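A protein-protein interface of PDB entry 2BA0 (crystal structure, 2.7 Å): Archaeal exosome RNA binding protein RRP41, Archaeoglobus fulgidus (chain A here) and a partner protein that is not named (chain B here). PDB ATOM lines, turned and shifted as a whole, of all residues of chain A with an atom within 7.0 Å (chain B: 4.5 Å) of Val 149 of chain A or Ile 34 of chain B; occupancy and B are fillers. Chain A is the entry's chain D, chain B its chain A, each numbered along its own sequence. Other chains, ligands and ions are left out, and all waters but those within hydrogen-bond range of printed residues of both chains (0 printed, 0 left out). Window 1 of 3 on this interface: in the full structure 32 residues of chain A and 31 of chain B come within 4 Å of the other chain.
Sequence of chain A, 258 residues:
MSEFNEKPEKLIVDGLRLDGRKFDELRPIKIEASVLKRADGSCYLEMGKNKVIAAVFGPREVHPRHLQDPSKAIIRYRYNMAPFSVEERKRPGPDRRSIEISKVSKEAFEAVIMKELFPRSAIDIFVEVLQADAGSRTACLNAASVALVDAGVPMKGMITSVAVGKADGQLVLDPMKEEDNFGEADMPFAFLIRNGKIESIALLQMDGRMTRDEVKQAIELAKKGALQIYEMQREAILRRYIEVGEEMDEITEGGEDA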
ATOM      1  N   ASP A  40       3.276  23.891 -24.908  1.00  0.00           N
ATOM      2  CA  ASP A  40       2.587  23.511 -26.145  1.00  0.00           C
ATOM      3  C   ASP A  40       1.627  22.325 -25.904  1.00  0.00           C
ATOM      4  O   ASP A  40       0.592  22.221 -26.557  1.00  0.00           O
ATOM      5  CB  ASP A  40       3.604  23.133 -27.230  1.00  0.00           C
ATOM      6  CG  ASP A  40       4.431  24.323 -27.711  1.00  0.00           C
ATOM      7  OD1 ASP A  40       3.842  25.307 -28.197  1.00  0.00           O
ATOM      8  OD2 ASP A  40       5.679  24.280 -27.616  1.00  0.00           O
ATOM      9  N   GLY A  41       1.988  21.441 -24.970  1.00  0.00           N
ATOM     10  CA  GLY A  41       1.171  20.288 -24.629  1.00  0.00           C
ATOM     11  C   GLY A  41       1.387  19.915 -23.163  1.00  0.00           C
ATOM     12  O   GLY A  41       2.466  20.131 -22.619  1.00  0.00           O
ATOM     13  N   VAL A  56       5.279  19.738 -22.831  1.00  0.00           N
ATOM     14  CA  VAL A  56       6.001  19.593 -24.090  1.00  0.00           C
ATOM     15  C   VAL A  56       6.133  20.939 -24.797  1.00  0.00           C
ATOM     16  O   VAL A  56       5.201  21.734 -24.807  1.00  0.00           O
ATOM     17  CB  VAL A  56       5.274  18.605 -25.028  1.00  0.00           C
ATOM     18  CG1 VAL A  56       5.734  18.801 -26.469  1.00  0.00           C
ATOM     19  CG2 VAL A  56       5.567  17.199 -24.603  1.00  0.00           C
ATOM     20  N   ALA A 143       1.905   9.956 -19.242  1.00  0.00           N
ATOM     21  CA  ALA A 143       1.582  11.378 -19.242  1.00  0.00           C
ATOM     22  C   ALA A 143       2.234  12.086 -20.437  1.00  0.00           C
ATOM     23  O   ALA A 143       1.630  12.975 -21.049  1.00  0.00           O
ATOM     24  CB  ALA A 143       2.010  12.012 -17.941  1.00  0.00           C
ATOM     25  N   ALA A 144       3.452  11.682 -20.788  1.00  0.00           N
ATOM     26  CA  ALA A 144       4.153  12.305 -21.916  1.00  0.00           C
ATOM     27  C   ALA A 144       3.403  12.041 -23.207  1.00  0.00           C
ATOM     28  O   ALA A 144       3.284  12.926 -24.052  1.00  0.00           O
ATOM     29  CB  ALA A 144       5.585  11.765 -22.033  1.00  0.00           C
ATOM     30  N   SER A 145       2.911  10.816 -23.362  1.00  0.00           N
ATOM     31  CA  SER A 145       2.184  10.448 -24.566  1.00  0.00           C
ATOM     32  C   SER A 145       0.963  11.361 -24.724  1.00  0.00           C
ATOM     33  O   SER A 145       0.756  11.966 -25.775  1.00  0.00           O
ATOM     34  CB  SER A 145       1.760   8.987 -24.488  1.00  0.00           C
ATOM     35  OG  SER A 145       1.124   8.589 -25.689  1.00  0.00           O
ATOM     36  N   VAL A 146       0.164  11.471 -23.671  1.00  0.00           N
ATOM     37  CA  VAL A 146      -0.990  12.349 -23.706  1.00  0.00           C
ATOM     38  C   VAL A 146      -0.577  13.794 -23.993  1.00  0.00           C
ATOM     39  O   VAL A 146      -1.273  14.503 -24.716  1.00  0.00           O
ATOM     40  CB  VAL A 146      -1.730  12.326 -22.373  1.00  0.00           C
ATOM     41  CG1 VAL A 146      -2.706  13.503 -22.294  1.00  0.00           C
ATOM     42  CG2 VAL A 146      -2.441  10.998 -22.212  1.00  0.00           C
ATOM     43  N   ALA A 147       0.550  14.229 -23.421  1.00  0.00           N
ATOM     44  CA  ALA A 147       1.041  15.604 -23.613  1.00  0.00           C
ATOM     45  C   ALA A 147       1.476  15.857 -25.036  1.00  0.00           C
ATOM     46  O   ALA A 147       1.287  16.948 -25.561  1.00  0.00           O
ATOM     47  CB  ALA A 147       2.195  15.889 -22.685  1.00  0.00           C
ATOM     48  N   LEU A 148       2.078  14.846 -25.655  1.00  0.00           N
ATOM     49  CA  LEU A 148       2.524  14.968 -27.030  1.00  0.00           C
ATOM     50  C   LEU A 148       1.322  15.078 -27.972  1.00  0.00           C
ATOM     51  O   LEU A 148       1.337  15.880 -28.908  1.00  0.00           O
ATOM     52  CB  LEU A 148       3.412  13.777 -27.393  1.00  0.00           C
ATOM     53  CG  LEU A 148       4.862  13.944 -26.927  1.00  0.00           C
ATOM     54  CD1 LEU A 148       5.566  12.592 -26.837  1.00  0.00           C
ATOM     55  CD2 LEU A 148       5.582  14.853 -27.900  1.00  0.00           C
ATOM     56  N   VAL A 149       0.289  14.276 -27.721  1.00  0.00           N
ATOM     57  CA  VAL A 149      -0.917  14.325 -28.529  1.00  0.00           C
ATOM     58  C   VAL A 149      -1.483  15.713 -28.320  1.00  0.00           C
ATOM     59  O   VAL A 149      -1.806  16.408 -29.268  1.00  0.00           O
ATOM     60  CB  VAL A 149      -1.968  13.291 -28.066  1.00  0.00           C
ATOM     61  CG1 VAL A 149      -3.306  13.555 -28.755  1.00  0.00           C
ATOM     62  CG2 VAL A 149      -1.492  11.887 -28.387  1.00  0.00           C
ATOM     63  N   ASP A 150      -1.579  16.110 -27.060  1.00  0.00           N
ATOM     64  CA  ASP A 150      -2.093  17.424 -26.668  1.00  0.00           C
ATOM     65  C   ASP A 150      -1.384  18.602 -27.341  1.00  0.00           C
ATOM     66  O   ASP A 150      -1.928  19.685 -27.402  1.00  0.00           O
ATOM     67  CB  ASP A 150      -1.978  17.578 -25.142  1.00  0.00           C
ATOM     68  CG  ASP A 150      -2.517  18.904 -24.644  1.00  0.00           C
ATOM     69  OD1 ASP A 150      -1.899  19.521 -23.736  1.00  0.00           O
ATOM     70  OD2 ASP A 150      -3.573  19.324 -25.157  1.00  0.00           O
ATOM     71  N   ALA A 151      -0.168  18.404 -27.832  1.00  0.00           N
ATOM     72  CA  ALA A 151       0.569  19.491 -28.482  1.00  0.00           C
ATOM     73  C   ALA A 151       0.445  19.402 -29.985  1.00  0.00           C
ATOM     74  O   ALA A 151       0.873  20.303 -30.706  1.00  0.00           O
ATOM     75  CB  ALA A 151       2.046  19.446 -28.097  1.00  0.00           C
ATOM     76  N   GLY A 152      -0.121  18.301 -30.458  1.00  0.00           N
ATOM     77  CA  GLY A 152      -0.285  18.139 -31.881  1.00  0.00           C
ATOM     78  C   GLY A 152       0.965  17.751 -32.653  1.00  0.00           C
ATOM     79  O   GLY A 152       1.121  18.191 -33.791  1.00  0.00           O
ATOM     80  N   VAL A 153       1.859  16.944 -32.075  1.00  0.00           N
ATOM     81  CA  VAL A 153       3.050  16.537 -32.828  1.00  0.00           C
ATOM     82  C   VAL A 153       2.715  15.196 -33.455  1.00  0.00           C
ATOM     83  O   VAL A 153       2.158  14.320 -32.800  1.00  0.00           O
ATOM     84  CB  VAL A 153       4.348  16.388 -31.946  1.00  0.00           C
ATOM     85  CG1 VAL A 153       4.383  17.446 -30.842  1.00  0.00           C
ATOM     86  CG2 VAL A 153       4.442  14.999 -31.369  1.00  0.00           C
ATOM     87  N   MET A 155       2.583  11.545 -34.561  1.00  0.00           N
ATOM     88  CA  MET A 155       3.079  10.308 -33.976  1.00  0.00           C
ATOM     89  C   MET A 155       2.471   9.138 -34.736  1.00  0.00           C
ATOM     90  O   MET A 155       1.445   9.298 -35.400  1.00  0.00           O
ATOM     91  CB  MET A 155       2.692  10.217 -32.504  1.00  0.00           C
ATOM     92  CG  MET A 155       3.234  11.339 -31.653  1.00  0.00           C
ATOM     93  SD  MET A 155       2.782  11.124 -29.935  1.00  0.00           S
ATOM     94  CE  MET A 155       1.298  12.069 -29.892  1.00  0.00           C
ATOM     95  N   GLY A 157       1.245   6.603 -33.327  1.00  0.00           N
ATOM     96  CA  GLY A 157       0.159   6.125 -32.494  1.00  0.00           C
ATOM     97  C   GLY A 157       0.452   6.545 -31.065  1.00  0.00           C
ATOM     98  O   GLY A 157       1.287   7.415 -30.842  1.00  0.00           O
ATOM     99  N   MET A 158      -0.212   5.934 -30.093  1.00  0.00           N
ATOM    100  CA  MET A 158       0.026   6.300 -28.713  1.00  0.00           C
ATOM    101  C   MET A 158       0.912   5.321 -27.997  1.00  0.00           C
ATOM    102  O   MET A 158       1.022   4.161 -28.398  1.00  0.00           O
ATOM    103  CB  MET A 158      -1.288   6.430 -27.967  1.00  0.00           C
ATOM    104  CG  MET A 158      -2.141   7.559 -28.499  1.00  0.00           C
ATOM    105  SD  MET A 158      -3.331   8.039 -27.281  1.00  0.00           S
ATOM    106  CE  MET A 158      -2.231   8.799 -26.043  1.00  0.00           C
ATOM    107  N   ILE A 159       1.555   5.805 -26.935  1.00  0.00           N
ATOM    108  CA  ILE A 159       2.436   4.978 -26.127  1.00  0.00           C
ATOM    109  C   ILE A 159       1.849   4.795 -24.742  1.00  0.00           C
ATOM    110  O   ILE A 159       1.522   5.771 -24.068  1.00  0.00           O
ATOM    111  CB  ILE A 159       3.829   5.589 -26.000  1.00  0.00           C
ATOM    112  CG1 ILE A 159       4.618   5.301 -27.271  1.00  0.00           C
ATOM    113  CG2 ILE A 159       4.539   5.021 -24.776  1.00  0.00           C
ATOM    114  CD1 ILE A 159       6.060   5.703 -27.192  1.00  0.00           C
ATOM    115  N   ILE A 237      -8.280  12.409 -23.254  1.00  0.00           N
ATOM    116  CA  ILE A 237      -8.081  13.299 -24.387  1.00  0.00           C
ATOM    117  C   ILE A 237      -9.386  13.765 -25.009  1.00  0.00           C
ATOM    118  O   ILE A 237      -9.604  14.965 -25.173  1.00  0.00           O
ATOM    119  CB  ILE A 237      -7.243  12.618 -25.501  1.00  0.00           C
ATOM    120  CG1 ILE A 237      -5.812  12.379 -25.011  1.00  0.00           C
ATOM    121  CG2 ILE A 237      -7.242  13.477 -26.766  1.00  0.00           C
ATOM    122  CD1 ILE A 237      -4.948  11.641 -26.013  1.00  0.00           C
ATOM    123  N   LEU A 238     -10.240  12.810 -25.375  1.00  0.00           N
ATOM    124  CA  LEU A 238     -11.515  13.121 -26.007  1.00  0.00           C
ATOM    125  C   LEU A 238     -12.343  14.025 -25.122  1.00  0.00           C
ATOM    126  O   LEU A 238     -12.848  15.052 -25.567  1.00  0.00           O
ATOM    127  CB  LEU A 238     -12.278  11.838 -26.305  1.00  0.00           C
ATOM    128  CG  LEU A 238     -11.642  10.911 -27.349  1.00  0.00           C
ATOM    129  CD1 LEU A 238     -12.420   9.596 -27.406  1.00  0.00           C
ATOM    130  CD2 LEU A 238     -11.613  11.596 -28.726  1.00  0.00           C
ATOM    131  N   TYR A 241     -11.223  17.334 -25.427  1.00  0.00           N
ATOM    132  CA  TYR A 241     -11.314  17.938 -26.751  1.00  0.00           C
ATOM    133  C   TYR A 241     -12.670  17.993 -27.422  1.00  0.00           C
ATOM    134  O   TYR A 241     -12.789  18.564 -28.508  1.00  0.00           O
ATOM    135  CB  TYR A 241     -10.342  17.257 -27.713  1.00  0.00           C
ATOM    136  CG  TYR A 241      -8.926  17.767 -27.618  1.00  0.00           C
ATOM    137  CD1 TYR A 241      -8.067  17.327 -26.610  1.00  0.00           C
ATOM    138  CD2 TYR A 241      -8.454  18.722 -28.513  1.00  0.00           C
ATOM    139  CE1 TYR A 241      -6.775  17.834 -26.494  1.00  0.00           C
ATOM    140  CE2 TYR A 241      -7.171  19.235 -28.405  1.00  0.00           C
ATOM    141  CZ  TYR A 241      -6.335  18.787 -27.394  1.00  0.00           C
ATOM    142  OH  TYR A 241      -5.064  19.301 -27.282  1.00  0.00           O
ATOM    143  N   VAL B   5     -10.611  11.934 -34.123  1.00  0.00           N
ATOM    144  CA  VAL B   5      -9.722  10.776 -34.136  1.00  0.00           C
ATOM    145  C   VAL B   5      -8.397  11.070 -33.424  1.00  0.00           C
ATOM    146  O   VAL B   5      -8.027  12.226 -33.217  1.00  0.00           O
ATOM    147  CB  VAL B   5      -9.435  10.297 -35.589  1.00  0.00           C
ATOM    148  CG1 VAL B   5     -10.646   9.588 -36.154  1.00  0.00           C
ATOM    149  CG2 VAL B   5      -9.104  11.473 -36.465  1.00  0.00           C
ATOM    150  N   LEU B   6      -7.697  10.013 -33.038  1.00  0.00           N
ATOM    151  CA  LEU B   6      -6.412  10.136 -32.362  1.00  0.00           C
ATOM    152  C   LEU B   6      -5.311   9.431 -33.166  1.00  0.00           C
ATOM    153  O   LEU B   6      -5.578   8.538 -33.986  1.00  0.00           O
ATOM    154  CB  LEU B   6      -6.488   9.512 -30.963  1.00  0.00           C
ATOM    155  CG  LEU B   6      -7.529  10.099 -30.007  1.00  0.00           C
ATOM    156  CD1 LEU B   6      -7.361   9.505 -28.614  1.00  0.00           C
ATOM    157  CD2 LEU B   6      -7.370  11.602 -29.962  1.00  0.00           C
ATOM    158  N   PRO B   7      -4.054   9.845 -32.962  1.00  0.00           N
ATOM    159  CA  PRO B   7      -2.971   9.192 -33.698  1.00  0.00           C
ATOM    160  C   PRO B   7      -3.007   7.678 -33.493  1.00  0.00           C
ATOM    161  O   PRO B   7      -3.213   7.186 -32.378  1.00  0.00           O
ATOM    162  CB  PRO B   7      -1.712   9.858 -33.136  1.00  0.00           C
ATOM    163  CG  PRO B   7      -2.191  10.587 -31.881  1.00  0.00           C
ATOM    164  CD  PRO B   7      -3.561  11.023 -32.232  1.00  0.00           C
ATOM    165  N   ILE B  33      -2.144  12.806 -36.000  1.00  0.00           N
ATOM    166  CA  ILE B  33      -2.399  13.940 -35.122  1.00  0.00           C
ATOM    167  C   ILE B  33      -3.845  13.901 -34.640  1.00  0.00           C
ATOM    168  O   ILE B  33      -4.690  13.259 -35.262  1.00  0.00           O
ATOM    169  CB  ILE B  33      -2.202  15.270 -35.851  1.00  0.00           C
ATOM    170  CG1 ILE B  33      -3.123  15.318 -37.074  1.00  0.00           C
ATOM    171  CG2 ILE B  33      -0.741  15.434 -36.250  1.00  0.00           C
ATOM    172  CD1 ILE B  33      -3.356  16.710 -37.655  1.00  0.00           C
ATOM    173  N   ILE B  34      -4.130  14.574 -33.527  1.00  0.00           N
ATOM    174  CA  ILE B  34      -5.494  14.630 -33.033  1.00  0.00           C
ATOM    175  C   ILE B  34      -6.252  15.590 -33.951  1.00  0.00           C
ATOM    176  O   ILE B  34      -5.695  16.585 -34.420  1.00  0.00           O
ATOM    177  CB  ILE B  34      -5.569  15.166 -31.581  1.00  0.00           C
ATOM    178  CG1 ILE B  34      -6.991  14.979 -31.041  1.00  0.00           C
ATOM    179  CG2 ILE B  34      -5.186  16.646 -31.531  1.00  0.00           C
ATOM    180  CD1 ILE B  34      -7.132  15.303 -29.581  1.00  0.00           C
ATOM    181  N   GLY B  35      -7.513  15.285 -34.224  1.00  0.00           N
ATOM    182  CA  GLY B  35      -8.292  16.158 -35.086  1.00  0.00           C
ATOM    183  C   GLY B  35      -9.581  15.533 -35.575  1.00  0.00           C
ATOM    184  O   GLY B  35      -9.943  14.423 -35.160  1.00  0.00           O
ATOM    185  N   VAL B  46      -7.274  14.597 -42.052  1.00  0.00           N
ATOM    186  CA  VAL B  46      -7.525  14.854 -40.643  1.00  0.00           C
ATOM    187  C   VAL B  46      -7.329  16.343 -40.416  1.00  0.00           C
ATOM    188  O   VAL B  46      -6.229  16.852 -40.570  1.00  0.00           O
ATOM    189  CB  VAL B  46      -6.556  14.098 -39.730  1.00  0.00           C
ATOM    190  CG1 VAL B  46      -6.656  14.651 -38.316  1.00  0.00           C
ATOM    191  CG2 VAL B  46      -6.879  12.619 -39.739  1.00  0.00           C
ATOM    192  N   ILE B  47      -8.409  17.037 -40.076  1.00  0.00           N
ATOM    193  CA  ILE B  47      -8.359  18.466 -39.820  1.00  0.00           C
ATOM    194  C   ILE B  47      -7.786  18.682 -38.429  1.00  0.00           C
ATOM    195  O   ILE B  47      -8.364  18.241 -37.438  1.00  0.00           O
ATOM    196  CB  ILE B  47      -9.757  19.073 -39.896  1.00  0.00           C
ATOM    197  CG1 ILE B  47     -10.338  18.830 -41.295  1.00  0.00           C
ATOM    198  CG2 ILE B  47      -9.696  20.563 -39.604  1.00  0.00           C
ATOM    199  CD1 ILE B  47     -11.769  19.300 -41.470  1.00  0.00           C
ATOM    200  N   PRO B  48      -6.638  19.379 -38.342  1.00  0.00           N
ATOM    201  CA  PRO B  48      -5.917  19.688 -37.099  1.00  0.00           C
ATOM    202  C   PRO B  48      -6.629  20.603 -36.106  1.00  0.00           C
ATOM    203  O   PRO B  48      -7.412  21.471 -36.479  1.00  0.00           O
ATOM    204  CB  PRO B  48      -4.610  20.289 -37.607  1.00  0.00           C
ATOM    205  CG  PRO B  48      -5.050  21.014 -38.827  1.00  0.00           C
ATOM    206  CD  PRO B  48      -5.977  20.021 -39.494  1.00  0.00           C
ATOM    207  N   LEU B  49      -6.332  20.400 -34.831  1.00  0.00           N
ATOM    208  CA  LEU B  49      -6.932  21.183 -33.767  1.00  0.00           C
ATOM    209  C   LEU B  49      -5.852  21.918 -32.988  1.00  0.00           C
ATOM    210  O   LEU B  49      -6.101  22.974 -32.404  1.00  0.00           O
ATOM    211  CB  LEU B  49      -7.717  20.261 -32.818  1.00  0.00           C
ATOM    212  CG  LEU B  49      -8.961  19.548 -33.368  1.00  0.00           C
ATOM    213  CD1 LEU B  49      -9.470  18.518 -32.378  1.00  0.00           C
ATOM    214  CD2 LEU B  49     -10.037  20.579 -33.667  1.00  0.00           C
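Of the 21 printed residues of chain A, 6 touch a printed residue of chain B.
Hydrophobic or aromatic side chains of chain A that line the printed part of chain B: Val 149, Ile 237 and Tyr 241.
Along chain A the printed residues that touch a printed residue of chain B span positions 149 to 241.
Hydrophobic or aromatic side chains of chain B that line the printed part of chain A: Leu 6, Pro 7 and Ile 34.
Among the printed residues, 8 pairs touch across the chains.
Among the printed residues, no Asp or Glu carboxylate lies within 4 Å of a Lys or Arg side-chain nitrogen of the other chain.
Printed residues of chain B within 4 Å of Val 149 of chain A: Pro 7 and Ile 34.
Of the printed residues of chain B, Ile 237 of chain A touches Leu 6 (3.7 Å) and Ile 34 (3.4 Å).
Of the printed residues of chain A, Leu 6 of chain B touches Ile 237 (3.7 Å).
Of the printed residues of chain B, Met 158 of chain A touches Pro 7 (3.97 Å).
Of the printed residues of chain B, Met 155 of chain A touches Pro 7 (3.9 Å).
The nearest printed residue of chain B that does not touch Val 149 of chain A is Leu 6 of chain B (4.7 Å).
The nearest residue of chain A that does not touch Ile 34 of chain B is Gly 152 of chain A (5.1 Å).
The nearest printed residue of chain B that does not touch Ile 237 of chain A is Pro 7 of chain B (6.4 Å).
CG2 of Val 149 of chain A touches CG of Pro 7 of chain B, at 3.8 Å.
Val 149 of chain A touches Ile 34 of chain B.
CB of Pro 7 of chain B touches O of Met 155 of chain A (3.9 Å).
Pro 7 of chain B touches Gly 157 of chain A (O to CA, 3.5 Å).
Met 158 of chain A touches Pro 7 of chain B.
Ile 237 of chain A touches Leu 6 of chain B (CG2 to CD2, 3.7 Å).
CD1 of Ile 34 of chain B touches CG2 of Ile 237 of chain A (3.4 Å).
Ile 34 of chain B touches Tyr 241 of chain A (CD1 to CG, 3.6 Å).
The side-chain carboxylate (OD2) of Asp 150 of chain A lies within hydrogen-bond range of the side-chain hydroxyl (OH) of Tyr 241 of chain A, at 2.6 Å.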
